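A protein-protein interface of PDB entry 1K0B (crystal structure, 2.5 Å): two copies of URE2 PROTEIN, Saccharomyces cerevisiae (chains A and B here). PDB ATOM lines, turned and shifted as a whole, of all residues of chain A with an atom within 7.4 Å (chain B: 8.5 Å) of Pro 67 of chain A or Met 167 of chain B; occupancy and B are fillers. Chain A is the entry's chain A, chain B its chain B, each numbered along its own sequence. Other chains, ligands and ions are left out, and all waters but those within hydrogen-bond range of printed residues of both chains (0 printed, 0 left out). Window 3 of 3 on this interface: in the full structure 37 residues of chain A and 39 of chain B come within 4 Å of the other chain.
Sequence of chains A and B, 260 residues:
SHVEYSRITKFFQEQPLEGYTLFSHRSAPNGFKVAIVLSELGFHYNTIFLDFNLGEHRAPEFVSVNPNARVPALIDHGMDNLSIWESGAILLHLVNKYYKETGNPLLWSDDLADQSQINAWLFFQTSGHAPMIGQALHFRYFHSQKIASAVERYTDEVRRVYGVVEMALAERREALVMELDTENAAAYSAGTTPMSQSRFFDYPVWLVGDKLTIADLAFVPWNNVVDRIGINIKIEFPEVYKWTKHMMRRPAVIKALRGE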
ATOM      1  N   HIS A  57      23.900 -44.429  21.631  1.00  0.00           N
ATOM      2  CA  HIS A  57      24.315 -43.159  21.050  1.00  0.00           C
ATOM      3  C   HIS A  57      23.680 -41.987  21.793  1.00  0.00           C
ATOM      4  O   HIS A  57      23.929 -40.828  21.465  1.00  0.00           O
ATOM      5  CB  HIS A  57      23.924 -43.106  19.571  1.00  0.00           C
ATOM      6  CG  HIS A  57      22.449 -43.193  19.335  1.00  0.00           C
ATOM      7  ND1 HIS A  57      21.663 -44.177  19.895  1.00  0.00           N
ATOM      8  CD2 HIS A  57      21.618 -42.424  18.593  1.00  0.00           C
ATOM      9  CE1 HIS A  57      20.412 -44.010  19.508  1.00  0.00           C
ATOM     10  NE2 HIS A  57      20.356 -42.954  18.718  1.00  0.00           N
ATOM     11  N   PHE A  62      28.469 -41.041  26.252  1.00  0.00           N
ATOM     12  CA  PHE A  62      28.740 -40.732  24.848  1.00  0.00           C
ATOM     13  C   PHE A  62      28.317 -39.321  24.438  1.00  0.00           C
ATOM     14  O   PHE A  62      28.907 -38.753  23.522  1.00  0.00           O
ATOM     15  CB  PHE A  62      28.056 -41.730  23.911  1.00  0.00           C
ATOM     16  CG  PHE A  62      28.329 -41.468  22.445  1.00  0.00           C
ATOM     17  CD1 PHE A  62      29.573 -41.763  21.891  1.00  0.00           C
ATOM     18  CD2 PHE A  62      27.349 -40.915  21.627  1.00  0.00           C
ATOM     19  CE1 PHE A  62      29.838 -41.516  20.545  1.00  0.00           C
ATOM     20  CE2 PHE A  62      27.604 -40.662  20.281  1.00  0.00           C
ATOM     21  CZ  PHE A  62      28.853 -40.966  19.738  1.00  0.00           C
ATOM     22  N   VAL A  63      27.294 -38.756  25.081  1.00  0.00           N
ATOM     23  CA  VAL A  63      26.879 -37.398  24.723  1.00  0.00           C
ATOM     24  C   VAL A  63      27.956 -36.443  25.234  1.00  0.00           C
ATOM     25  O   VAL A  63      28.074 -35.303  24.773  1.00  0.00           O
ATOM     26  CB  VAL A  63      25.488 -36.999  25.332  1.00  0.00           C
ATOM     27  CG1 VAL A  63      24.408 -37.981  24.878  1.00  0.00           C
ATOM     28  CG2 VAL A  63      25.563 -36.944  26.843  1.00  0.00           C
ATOM     29  N   SER A  64      28.748 -36.933  26.184  1.00  0.00           N
ATOM     30  CA  SER A  64      29.840 -36.161  26.762  1.00  0.00           C
ATOM     31  C   SER A  64      30.909 -36.024  25.691  1.00  0.00           C
ATOM     32  O   SER A  64      31.666 -35.046  25.666  1.00  0.00           O
ATOM     33  CB  SER A  64      30.406 -36.888  27.983  1.00  0.00           C
ATOM     34  OG  SER A  64      29.378 -37.143  28.931  1.00  0.00           O
ATOM     35  N   VAL A  65      30.953 -37.026  24.813  1.00  0.00           N
ATOM     36  CA  VAL A  65      31.888 -37.079  23.690  1.00  0.00           C
ATOM     37  C   VAL A  65      31.309 -36.298  22.511  1.00  0.00           C
ATOM     38  O   VAL A  65      31.966 -35.425  21.954  1.00  0.00           O
ATOM     39  CB  VAL A  65      32.138 -38.535  23.239  1.00  0.00           C
ATOM     40  CG1 VAL A  65      32.688 -38.555  21.824  1.00  0.00           C
ATOM     41  CG2 VAL A  65      33.110 -39.208  24.188  1.00  0.00           C
ATOM     42  N   ASN A  66      30.080 -36.628  22.129  1.00  0.00           N
ATOM     43  CA  ASN A  66      29.417 -35.935  21.036  1.00  0.00           C
ATOM     44  C   ASN A  66      28.095 -35.375  21.543  1.00  0.00           C
ATOM     45  O   ASN A  66      27.114 -36.112  21.702  1.00  0.00           O
ATOM     46  CB  ASN A  66      29.170 -36.873  19.857  1.00  0.00           C
ATOM     47  CG  ASN A  66      28.670 -36.136  18.630  1.00  0.00           C
ATOM     48  OD1 ASN A  66      28.663 -36.677  17.524  1.00  0.00           O
ATOM     49  ND2 ASN A  66      28.248 -34.887  18.820  1.00  0.00           N
ATOM     50  N   PRO A  67      28.052 -34.058  21.810  1.00  0.00           N
ATOM     51  CA  PRO A  67      26.828 -33.424  22.306  1.00  0.00           C
ATOM     52  C   PRO A  67      25.639 -33.671  21.406  1.00  0.00           C
ATOM     53  O   PRO A  67      24.503 -33.725  21.874  1.00  0.00           O
ATOM     54  CB  PRO A  67      27.210 -31.944  22.397  1.00  0.00           C
ATOM     55  CG  PRO A  67      28.270 -31.792  21.352  1.00  0.00           C
ATOM     56  CD  PRO A  67      29.093 -33.049  21.552  1.00  0.00           C
ATOM     57  N   ASN A  68      25.903 -33.830  20.115  1.00  0.00           N
ATOM     58  CA  ASN A  68      24.848 -34.079  19.135  1.00  0.00           C
ATOM     59  C   ASN A  68      24.334 -35.527  19.202  1.00  0.00           C
ATOM     60  O   ASN A  68      23.317 -35.860  18.602  1.00  0.00           O
ATOM     61  CB  ASN A  68      25.368 -33.771  17.734  1.00  0.00           C
ATOM     62  CG  ASN A  68      24.284 -33.837  16.683  1.00  0.00           C
ATOM     63  OD1 ASN A  68      24.542 -34.198  15.537  1.00  0.00           O
ATOM     64  ND2 ASN A  68      23.066 -33.471  17.061  1.00  0.00           N
ATOM     65  N   ALA A  69      25.052 -36.387  19.921  1.00  0.00           N
ATOM     66  CA  ALA A  69      24.657 -37.786  20.100  1.00  0.00           C
ATOM     67  C   ALA A  69      24.523 -38.578  18.797  1.00  0.00           C
ATOM     68  O   ALA A  69      23.550 -39.299  18.580  1.00  0.00           O
ATOM     69  CB  ALA A  69      23.345 -37.850  20.894  1.00  0.00           C
ATOM     70  N   ARG A  70      25.520 -38.457  17.938  1.00  0.00           N
ATOM     71  CA  ARG A  70      25.512 -39.155  16.658  1.00  0.00           C
ATOM     72  C   ARG A  70      26.934 -39.638  16.403  1.00  0.00           C
ATOM     73  O   ARG A  70      27.872 -39.168  17.042  1.00  0.00           O
ATOM     74  CB  ARG A  70      25.097 -38.187  15.526  1.00  0.00           C
ATOM     75  CG  ARG A  70      23.670 -37.639  15.604  1.00  0.00           C
ATOM     76  CD  ARG A  70      22.671 -38.755  15.390  1.00  0.00           C
ATOM     77  NE  ARG A  70      21.270 -38.328  15.341  1.00  0.00           N
ATOM     78  CZ  ARG A  70      20.492 -38.116  16.402  1.00  0.00           C
ATOM     79  NH1 ARG A  70      20.962 -38.279  17.638  1.00  0.00           N
ATOM     80  NH2 ARG A  70      19.222 -37.771  16.223  1.00  0.00           N
ATOM     81  N   SER A  83      37.956 -34.734  22.043  1.00  0.00           N
ATOM     82  CA  SER A  83      36.822 -35.250  21.282  1.00  0.00           C
ATOM     83  C   SER A  83      36.500 -34.334  20.107  1.00  0.00           C
ATOM     84  O   SER A  83      36.267 -33.136  20.285  1.00  0.00           O
ATOM     85  CB  SER A  83      35.569 -35.363  22.157  1.00  0.00           C
ATOM     86  OG  SER A  83      35.721 -36.342  23.162  1.00  0.00           O
ATOM     87  N   TRP A  85      33.795 -34.230  17.020  1.00  0.00           N
ATOM     88  CA  TRP A  85      32.599 -34.975  16.651  1.00  0.00           C
ATOM     89  C   TRP A  85      31.972 -34.937  15.262  1.00  0.00           C
ATOM     90  O   TRP A  85      31.296 -35.900  14.900  1.00  0.00           O
ATOM     91  CB  TRP A  85      31.486 -34.770  17.697  1.00  0.00           C
ATOM     92  CG  TRP A  85      31.334 -33.383  18.229  1.00  0.00           C
ATOM     93  CD1 TRP A  85      32.114 -32.775  19.168  1.00  0.00           C
ATOM     94  CD2 TRP A  85      30.320 -32.435  17.873  1.00  0.00           C
ATOM     95  NE1 TRP A  85      31.648 -31.506  19.422  1.00  0.00           N
ATOM     96  CE2 TRP A  85      30.546 -31.274  18.640  1.00  0.00           C
ATOM     97  CE3 TRP A  85      29.239 -32.458  16.980  1.00  0.00           C
ATOM     98  CZ2 TRP A  85      29.731 -30.140  18.544  1.00  0.00           C
ATOM     99  CZ3 TRP A  85      28.427 -31.329  16.885  1.00  0.00           C
ATOM    100  CH2 TRP A  85      28.679 -30.187  17.664  1.00  0.00           C
ATOM    101  N   GLN B 117      37.388 -28.038  17.806  1.00  0.00           N
ATOM    102  CA  GLN B 117      36.094 -27.813  18.438  1.00  0.00           C
ATOM    103  C   GLN B 117      35.270 -26.826  17.594  1.00  0.00           C
ATOM    104  O   GLN B 117      34.080 -27.038  17.363  1.00  0.00           O
ATOM    105  CB  GLN B 117      36.272 -27.276  19.863  1.00  0.00           C
ATOM    106  CG  GLN B 117      36.957 -28.246  20.832  1.00  0.00           C
ATOM    107  CD  GLN B 117      36.491 -29.687  20.652  1.00  0.00           C
ATOM    108  OE1 GLN B 117      36.826 -30.344  19.659  1.00  0.00           O
ATOM    109  NE2 GLN B 117      35.705 -30.182  21.603  1.00  0.00           N
ATOM    110  N   ALA B 120      33.880 -28.534  14.656  1.00  0.00           N
ATOM    111  CA  ALA B 120      32.783 -29.417  14.981  1.00  0.00           C
ATOM    112  C   ALA B 120      31.505 -28.605  14.851  1.00  0.00           C
ATOM    113  O   ALA B 120      30.678 -28.890  13.990  1.00  0.00           O
ATOM    114  CB  ALA B 120      32.945 -29.955  16.388  1.00  0.00           C
ATOM    115  N   TRP B 121      31.372 -27.564  15.677  1.00  0.00           N
ATOM    116  CA  TRP B 121      30.191 -26.702  15.655  1.00  0.00           C
ATOM    117  C   TRP B 121      29.904 -26.108  14.279  1.00  0.00           C
ATOM    118  O   TRP B 121      28.745 -25.920  13.918  1.00  0.00           O
ATOM    119  CB  TRP B 121      30.329 -25.566  16.675  1.00  0.00           C
ATOM    120  CG  TRP B 121      30.340 -26.046  18.087  1.00  0.00           C
ATOM    121  CD1 TRP B 121      31.429 -26.165  18.903  1.00  0.00           C
ATOM    122  CD2 TRP B 121      29.223 -26.555  18.830  1.00  0.00           C
ATOM    123  NE1 TRP B 121      31.060 -26.723  20.107  1.00  0.00           N
ATOM    124  CE2 TRP B 121      29.713 -26.974  20.089  1.00  0.00           C
ATOM    125  CE3 TRP B 121      27.858 -26.701  18.556  1.00  0.00           C
ATOM    126  CZ2 TRP B 121      28.883 -27.531  21.073  1.00  0.00           C
ATOM    127  CZ3 TRP B 121      27.034 -27.255  19.535  1.00  0.00           C
ATOM    128  CH2 TRP B 121      27.552 -27.663  20.778  1.00  0.00           C
ATOM    129  N   PHE B 124      28.473 -28.869  12.065  1.00  0.00           N
ATOM    130  CA  PHE B 124      27.191 -29.161  12.660  1.00  0.00           C
ATOM    131  C   PHE B 124      26.147 -28.135  12.167  1.00  0.00           C
ATOM    132  O   PHE B 124      25.060 -28.498  11.716  1.00  0.00           O
ATOM    133  CB  PHE B 124      27.336 -29.104  14.183  1.00  0.00           C
ATOM    134  CG  PHE B 124      26.069 -29.381  14.922  1.00  0.00           C
ATOM    135  CD1 PHE B 124      25.282 -30.482  14.589  1.00  0.00           C
ATOM    136  CD2 PHE B 124      25.656 -28.541  15.951  1.00  0.00           C
ATOM    137  CE1 PHE B 124      24.090 -30.747  15.272  1.00  0.00           C
ATOM    138  CE2 PHE B 124      24.467 -28.788  16.644  1.00  0.00           C
ATOM    139  CZ  PHE B 124      23.679 -29.897  16.304  1.00  0.00           C
ATOM    140  N   ARG B 160      15.476 -30.209  18.182  1.00  0.00           N
ATOM    141  CA  ARG B 160      16.448 -31.092  18.795  1.00  0.00           C
ATOM    142  C   ARG B 160      17.845 -30.466  18.685  1.00  0.00           C
ATOM    143  O   ARG B 160      18.555 -30.336  19.688  1.00  0.00           O
ATOM    144  CB  ARG B 160      16.423 -32.448  18.096  1.00  0.00           C
ATOM    145  CG  ARG B 160      17.458 -33.415  18.614  1.00  0.00           C
ATOM    146  CD  ARG B 160      17.629 -34.611  17.691  1.00  0.00           C
ATOM    147  NE  ARG B 160      19.000 -35.087  17.774  1.00  0.00           N
ATOM    148  CZ  ARG B 160      20.017 -34.580  17.085  1.00  0.00           C
ATOM    149  NH1 ARG B 160      19.839 -33.584  16.229  1.00  0.00           N
ATOM    150  NH2 ARG B 160      21.233 -35.049  17.283  1.00  0.00           N
ATOM    151  N   VAL B 161      18.245 -30.073  17.476  1.00  0.00           N
ATOM    152  CA  VAL B 161      19.564 -29.474  17.308  1.00  0.00           C
ATOM    153  C   VAL B 161      19.700 -28.205  18.150  1.00  0.00           C
ATOM    154  O   VAL B 161      20.792 -27.900  18.636  1.00  0.00           O
ATOM    155  CB  VAL B 161      19.895 -29.145  15.815  1.00  0.00           C
ATOM    156  CG1 VAL B 161      19.701 -30.379  14.955  1.00  0.00           C
ATOM    157  CG2 VAL B 161      19.051 -27.994  15.309  1.00  0.00           C
ATOM    158  N   TYR B 162      18.614 -27.456  18.333  1.00  0.00           N
ATOM    159  CA  TYR B 162      18.718 -26.259  19.161  1.00  0.00           C
ATOM    160  C   TYR B 162      18.940 -26.673  20.609  1.00  0.00           C
ATOM    161  O   TYR B 162      19.672 -26.013  21.340  1.00  0.00           O
ATOM    162  CB  TYR B 162      17.477 -25.362  19.049  1.00  0.00           C
ATOM    163  CG  TYR B 162      17.645 -24.276  18.014  1.00  0.00           C
ATOM    164  CD1 TYR B 162      17.357 -24.515  16.676  1.00  0.00           C
ATOM    165  CD2 TYR B 162      18.182 -23.035  18.358  1.00  0.00           C
ATOM    166  CE1 TYR B 162      17.605 -23.559  15.701  1.00  0.00           C
ATOM    167  CE2 TYR B 162      18.435 -22.066  17.388  1.00  0.00           C
ATOM    168  CZ  TYR B 162      18.146 -22.338  16.059  1.00  0.00           C
ATOM    169  OH  TYR B 162      18.413 -21.407  15.080  1.00  0.00           O
ATOM    170  N   GLY B 163      18.320 -27.773  21.016  1.00  0.00           N
ATOM    171  CA  GLY B 163      18.504 -28.260  22.374  1.00  0.00           C
ATOM    172  C   GLY B 163      19.966 -28.578  22.643  1.00  0.00           C
ATOM    173  O   GLY B 163      20.468 -28.347  23.738  1.00  0.00           O
ATOM    174  N   VAL B 164      20.660 -29.100  21.637  1.00  0.00           N
ATOM    175  CA  VAL B 164      22.071 -29.439  21.779  1.00  0.00           C
ATOM    176  C   VAL B 164      22.890 -28.172  22.056  1.00  0.00           C
ATOM    177  O   VAL B 164      23.706 -28.131  22.985  1.00  0.00           O
ATOM    178  CB  VAL B 164      22.608 -30.147  20.495  1.00  0.00           C
ATOM    179  CG1 VAL B 164      24.108 -30.397  20.615  1.00  0.00           C
ATOM    180  CG2 VAL B 164      21.859 -31.466  20.271  1.00  0.00           C
ATOM    181  N   VAL B 165      22.666 -27.136  21.255  1.00  0.00           N
ATOM    182  CA  VAL B 165      23.379 -25.878  21.434  1.00  0.00           C
ATOM    183  C   VAL B 165      23.011 -25.296  22.800  1.00  0.00           C
ATOM    184  O   VAL B 165      23.870 -24.768  23.515  1.00  0.00           O
ATOM    185  CB  VAL B 165      23.009 -24.862  20.324  1.00  0.00           C
ATOM    186  CG1 VAL B 165      23.746 -23.542  20.547  1.00  0.00           C
ATOM    187  CG2 VAL B 165      23.346 -25.449  18.958  1.00  0.00           C
ATOM    188  N   GLU B 166      21.733 -25.409  23.158  1.00  0.00           N
ATOM    189  CA  GLU B 166      21.242 -24.911  24.437  1.00  0.00           C
ATOM    190  C   GLU B 166      21.951 -25.632  25.579  1.00  0.00           C
ATOM    191  O   GLU B 166      22.424 -25.002  26.518  1.00  0.00           O
ATOM    192  CB  GLU B 166      19.732 -25.143  24.559  1.00  0.00           C
ATOM    193  CG  GLU B 166      19.145 -24.653  25.870  1.00  0.00           C
ATOM    194  CD  GLU B 166      19.000 -23.145  25.905  1.00  0.00           C
ATOM    195  OE1 GLU B 166      18.721 -22.585  26.995  1.00  0.00           O
ATOM    196  OE2 GLU B 166      19.159 -22.522  24.833  1.00  0.00           O
ATOM    197  N   MET B 167      22.004 -26.958  25.494  1.00  0.00           N
ATOM    198  CA  MET B 167      22.660 -27.771  26.513  1.00  0.00           C
ATOM    199  C   MET B 167      24.136 -27.397  26.602  1.00  0.00           C
ATOM    200  O   MET B 167      24.697 -27.302  27.690  1.00  0.00           O
ATOM    201  CB  MET B 167      22.519 -29.265  26.173  1.00  0.00           C
ATOM    202  CG  MET B 167      23.406 -30.192  27.015  1.00  0.00           C
ATOM    203  SD  MET B 167      23.213 -31.973  26.657  1.00  0.00           S
ATOM    204  CE  MET B 167      24.042 -32.088  25.025  1.00  0.00           C
ATOM    205  N   ALA B 168      24.762 -27.178  25.453  1.00  0.00           N
ATOM    206  CA  ALA B 168      26.169 -26.821  25.424  1.00  0.00           C
ATOM    207  C   ALA B 168      26.410 -25.465  26.079  1.00  0.00           C
ATOM    208  O   ALA B 168      27.318 -25.318  26.891  1.00  0.00           O
ATOM    209  CB  ALA B 168      26.673 -26.813  23.990  1.00  0.00           C
ATOM    210  N   LEU B 169      25.597 -24.475  25.728  1.00  0.00           N
ATOM    211  CA  LEU B 169      25.757 -23.144  26.300  1.00  0.00           C
ATOM    212  C   LEU B 169      25.446 -23.125  27.793  1.00  0.00           C
ATOM    213  O   LEU B 169      25.994 -22.311  28.539  1.00  0.00           O
ATOM    214  CB  LEU B 169      24.865 -22.138  25.568  1.00  0.00           C
ATOM    215  CG  LEU B 169      25.279 -21.771  24.141  1.00  0.00           C
ATOM    216  CD1 LEU B 169      24.286 -20.765  23.577  1.00  0.00           C
ATOM    217  CD2 LEU B 169      26.696 -21.196  24.144  1.00  0.00           C
ATOM    218  N   ALA B 170      24.568 -24.021  28.225  1.00  0.00           N
ATOM    219  CA  ALA B 170      24.200 -24.106  29.631  1.00  0.00           C
ATOM    220  C   ALA B 170      25.382 -24.657  30.416  1.00  0.00           C
ATOM    221  O   ALA B 170      25.661 -24.219  31.528  1.00  0.00           O
ATOM    222  CB  ALA B 170      22.990 -25.006  29.802  1.00  0.00           C
ATOM    223  N   GLU B 171      26.080 -25.619  29.825  1.00  0.00           N
ATOM    224  CA  GLU B 171      27.240 -26.214  30.476  1.00  0.00           C
ATOM    225  C   GLU B 171      28.387 -25.216  30.583  1.00  0.00           C
ATOM    226  O   GLU B 171      29.140 -25.238  31.552  1.00  0.00           O
ATOM    227  CB  GLU B 171      27.698 -27.465  29.721  1.00  0.00           C
ATOM    228  CG  GLU B 171      26.795 -28.678  29.941  1.00  0.00           C
ATOM    229  CD  GLU B 171      27.253 -29.909  29.166  1.00  0.00           C
ATOM    230  OE1 GLU B 171      28.455 -30.264  29.254  1.00  0.00           O
ATOM    231  OE2 GLU B 171      26.410 -30.529  28.473  1.00  0.00           O
ATOM    232  N   ARG B 172      28.521 -24.344  29.587  1.00  0.00           N
ATOM    233  CA  ARG B 172      29.578 -23.337  29.605  1.00  0.00           C
ATOM    234  C   ARG B 172      29.223 -22.343  30.708  1.00  0.00           C
ATOM    235  O   ARG B 172      30.094 -21.831  31.411  1.00  0.00           O
ATOM    236  CB  ARG B 172      29.655 -22.597  28.264  1.00  0.00           C
ATOM    237  CG  ARG B 172      29.756 -23.477  27.019  1.00  0.00           C
ATOM    238  CD  ARG B 172      31.175 -23.933  26.732  1.00  0.00           C
ATOM    239  NE  ARG B 172      31.287 -24.650  25.456  1.00  0.00           N
ATOM    240  CZ  ARG B 172      30.772 -25.857  25.205  1.00  0.00           C
ATOM    241  NH1 ARG B 172      30.090 -26.512  26.140  1.00  0.00           N
ATOM    242  NH2 ARG B 172      30.957 -26.424  24.017  1.00  0.00           N
ATOM    243  N   ARG B 173      27.929 -22.080  30.846  1.00  0.00           N
ATOM    244  CA  ARG B 173      27.413 -21.149  31.847  1.00  0.00           C
ATOM    245  C   ARG B 173      27.806 -21.557  33.267  1.00  0.00           C
ATOM    246  O   ARG B 173      28.385 -20.767  34.013  1.00  0.00           O
ATOM    247  CB  ARG B 173      25.892 -21.079  31.734  1.00  0.00           C
ATOM    248  CG  ARG B 173      25.211 -20.263  32.807  1.00  0.00           C
ATOM    249  CD  ARG B 173      24.473 -19.111  32.178  1.00  0.00           C
ATOM    250  NE  ARG B 173      25.324 -17.937  32.070  1.00  0.00           N
ATOM    251  CZ  ARG B 173      25.300 -17.085  31.057  1.00  0.00           C
ATOM    252  NH1 ARG B 173      26.107 -16.042  31.067  1.00  0.00           N
ATOM    253  NH2 ARG B 173      24.491 -17.283  30.025  1.00  0.00           N
ATOM    254  N   GLU B 174      27.469 -22.790  33.630  1.00  0.00           N
ATOM    255  CA  GLU B 174      27.785 -23.341  34.942  1.00  0.00           C
ATOM    256  C   GLU B 174      29.292 -23.282  35.206  1.00  0.00           C
ATOM    257  O   GLU B 174      29.727 -22.967  36.311  1.00  0.00           O
ATOM    258  CB  GLU B 174      27.294 -24.788  35.007  1.00  0.00           C
ATOM    259  CG  GLU B 174      27.841 -25.608  36.159  1.00  0.00           C
ATOM    260  CD  GLU B 174      27.482 -27.082  36.032  1.00  0.00           C
ATOM    261  OE1 GLU B 174      26.273 -27.410  36.056  1.00  0.00           O
ATOM    262  OE2 GLU B 174      28.412 -27.910  35.899  1.00  0.00           O
ATOM    263  N   LEU B 207      30.667 -20.860  22.578  1.00  0.00           N
ATOM    264  CA  LEU B 207      30.829 -22.285  22.314  1.00  0.00           C
ATOM    265  C   LEU B 207      32.231 -22.849  22.560  1.00  0.00           C
ATOM    266  O   LEU B 207      32.360 -23.959  23.073  1.00  0.00           O
ATOM    267  CB  LEU B 207      30.385 -22.611  20.882  1.00  0.00           C
ATOM    268  CG  LEU B 207      28.884 -22.467  20.602  1.00  0.00           C
ATOM    269  CD1 LEU B 207      28.602 -22.730  19.123  1.00  0.00           C
ATOM    270  CD2 LEU B 207      28.099 -23.433  21.476  1.00  0.00           C
ATOM    271  N   PHE B 237      14.426 -21.600  24.326  1.00  0.00           N
ATOM    272  CA  PHE B 237      15.882 -21.703  24.449  1.00  0.00           C
ATOM    273  C   PHE B 237      16.560 -20.440  24.989  1.00  0.00           C
ATOM    274  O   PHE B 237      17.248 -19.724  24.259  1.00  0.00           O
ATOM    275  CB  PHE B 237      16.491 -22.092  23.088  1.00  0.00           C
ATOM    276  CG  PHE B 237      15.865 -23.317  22.471  1.00  0.00           C
ATOM    277  CD1 PHE B 237      14.893 -23.198  21.486  1.00  0.00           C
ATOM    278  CD2 PHE B 237      16.212 -24.588  22.913  1.00  0.00           C
ATOM    279  CE1 PHE B 237      14.273 -24.330  20.946  1.00  0.00           C
ATOM    280  CE2 PHE B 237      15.601 -25.722  22.384  1.00  0.00           C
ATOM    281  CZ  PHE B 237      14.629 -25.594  21.398  1.00  0.00           C
ATOM    282  N   GLU B 239      19.293 -19.710  26.950  1.00  0.00           N
ATOM    283  CA  GLU B 239      20.723 -19.496  26.711  1.00  0.00           C
ATOM    284  C   GLU B 239      20.962 -19.078  25.261  1.00  0.00           C
ATOM    285  O   GLU B 239      21.714 -18.138  25.001  1.00  0.00           O
ATOM    286  CB  GLU B 239      21.540 -20.757  27.031  1.00  0.00           C
ATOM    287  CG  GLU B 239      21.587 -21.149  28.511  1.00  0.00           C
ATOM    288  CD  GLU B 239      22.223 -20.082  29.402  1.00  0.00           C
ATOM    289  OE1 GLU B 239      23.333 -19.607  29.077  1.00  0.00           O
ATOM    290  OE2 GLU B 239      21.616 -19.724  30.436  1.00  0.00           O
ATOM    291  N   VAL B 240      20.308 -19.759  24.319  1.00  0.00           N
ATOM    292  CA  VAL B 240      20.474 -19.411  22.910  1.00  0.00           C
ATOM    293  C   VAL B 240      20.018 -17.975  22.656  1.00  0.00           C
ATOM    294  O   VAL B 240      20.564 -17.281  21.792  1.00  0.00           O
ATOM    295  CB  VAL B 240      19.694 -20.373  21.976  1.00  0.00           C
ATOM    296  CG1 VAL B 240      19.678 -19.821  20.556  1.00  0.00           C
ATOM    297  CG2 VAL B 240      20.350 -21.741  21.977  1.00  0.00           C
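The guanidinium group (NH2) of Arg 70 of chain A lies close to the guanidinium group (NE) of Arg 160 of chain B, 3.1 Å away.
ND2 of Asn 68 of chain A lies close to NH2 of Arg 160 of chain B.
The side-chain amide oxygen of Gln 117 of chain B sits close to the backbone carbonyl oxygen of Ser 83 of chain A, 2.9 Å away.
The backbone NH of Asn 68 of chain A lies close to the side-chain amide nitrogen of Asn 66 of chain A (2.9 Å).
The side-chain amide oxygen (OD1) of Asn 66 of chain A lies close to the backbone carbonyl oxygen (O) of Arg 70 of chain A.
Among the printed residues, merely in contact across the chains: Pro 67 of chain A with Val 164 of chain B, Pro 67 of chain A with Met 167 of chain B, Asn 68 of chain A with Phe 124 of chain B, Asn 68 of chain A with Val 164 of chain B, Trp 85 of chain A with Ala 120 of chain B, Trp 85 of chain A with Trp 121 of chain B and Trp 85 of chain A with Phe 124 of chain B.
Of the printed residues of chain B, Asn 68 of chain A touches Phe 124 (3.4 Å), Arg 160 (2.4 Å) and Val 164 (3.9 Å).
Printed residues of chain B within 4 Å of Arg 70 of chain A: Arg 160 (3.1 Å).
Printed residues of chain A within 4 Å of Gln 117 of chain B: Ser 83 (2.9 Å).
Printed residues of chain A within 4 Å of Val 164 of chain B: Pro 67 and Asn 68.
Arg 172 of chain B touches none of the printed residues of chain A.
Glu 239 of chain B touches none of the printed residues of chain A.
The nearest residue of chain B that does not touch Pro 67 of chain A is Trp 121 of chain B (4.2 Å).
The nearest residue of chain A that does not touch Met 167 of chain B is Val 63 of chain A (5.1 Å).
Of the 23 printed residues of chain B, 7 touch a printed residue of chain A.
Printed residues of chain B that touch a printed residue of chain A: Gln 117, Ala 120, Trp 121, Phe 124, Arg 160, Val 164 and Met 167.
Of the 12 printed residues of chain A, 5 touch a printed residue of chain B.
Among the printed residues, no Asp or Glu carboxylate lies within 4 Å of a Lys or Arg side-chain nitrogen of the other chain.
No position is printed for both chains.
Of the 10 pairs that touch across the chains among the printed residues, none has its exchanged pair printed and touching as well.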
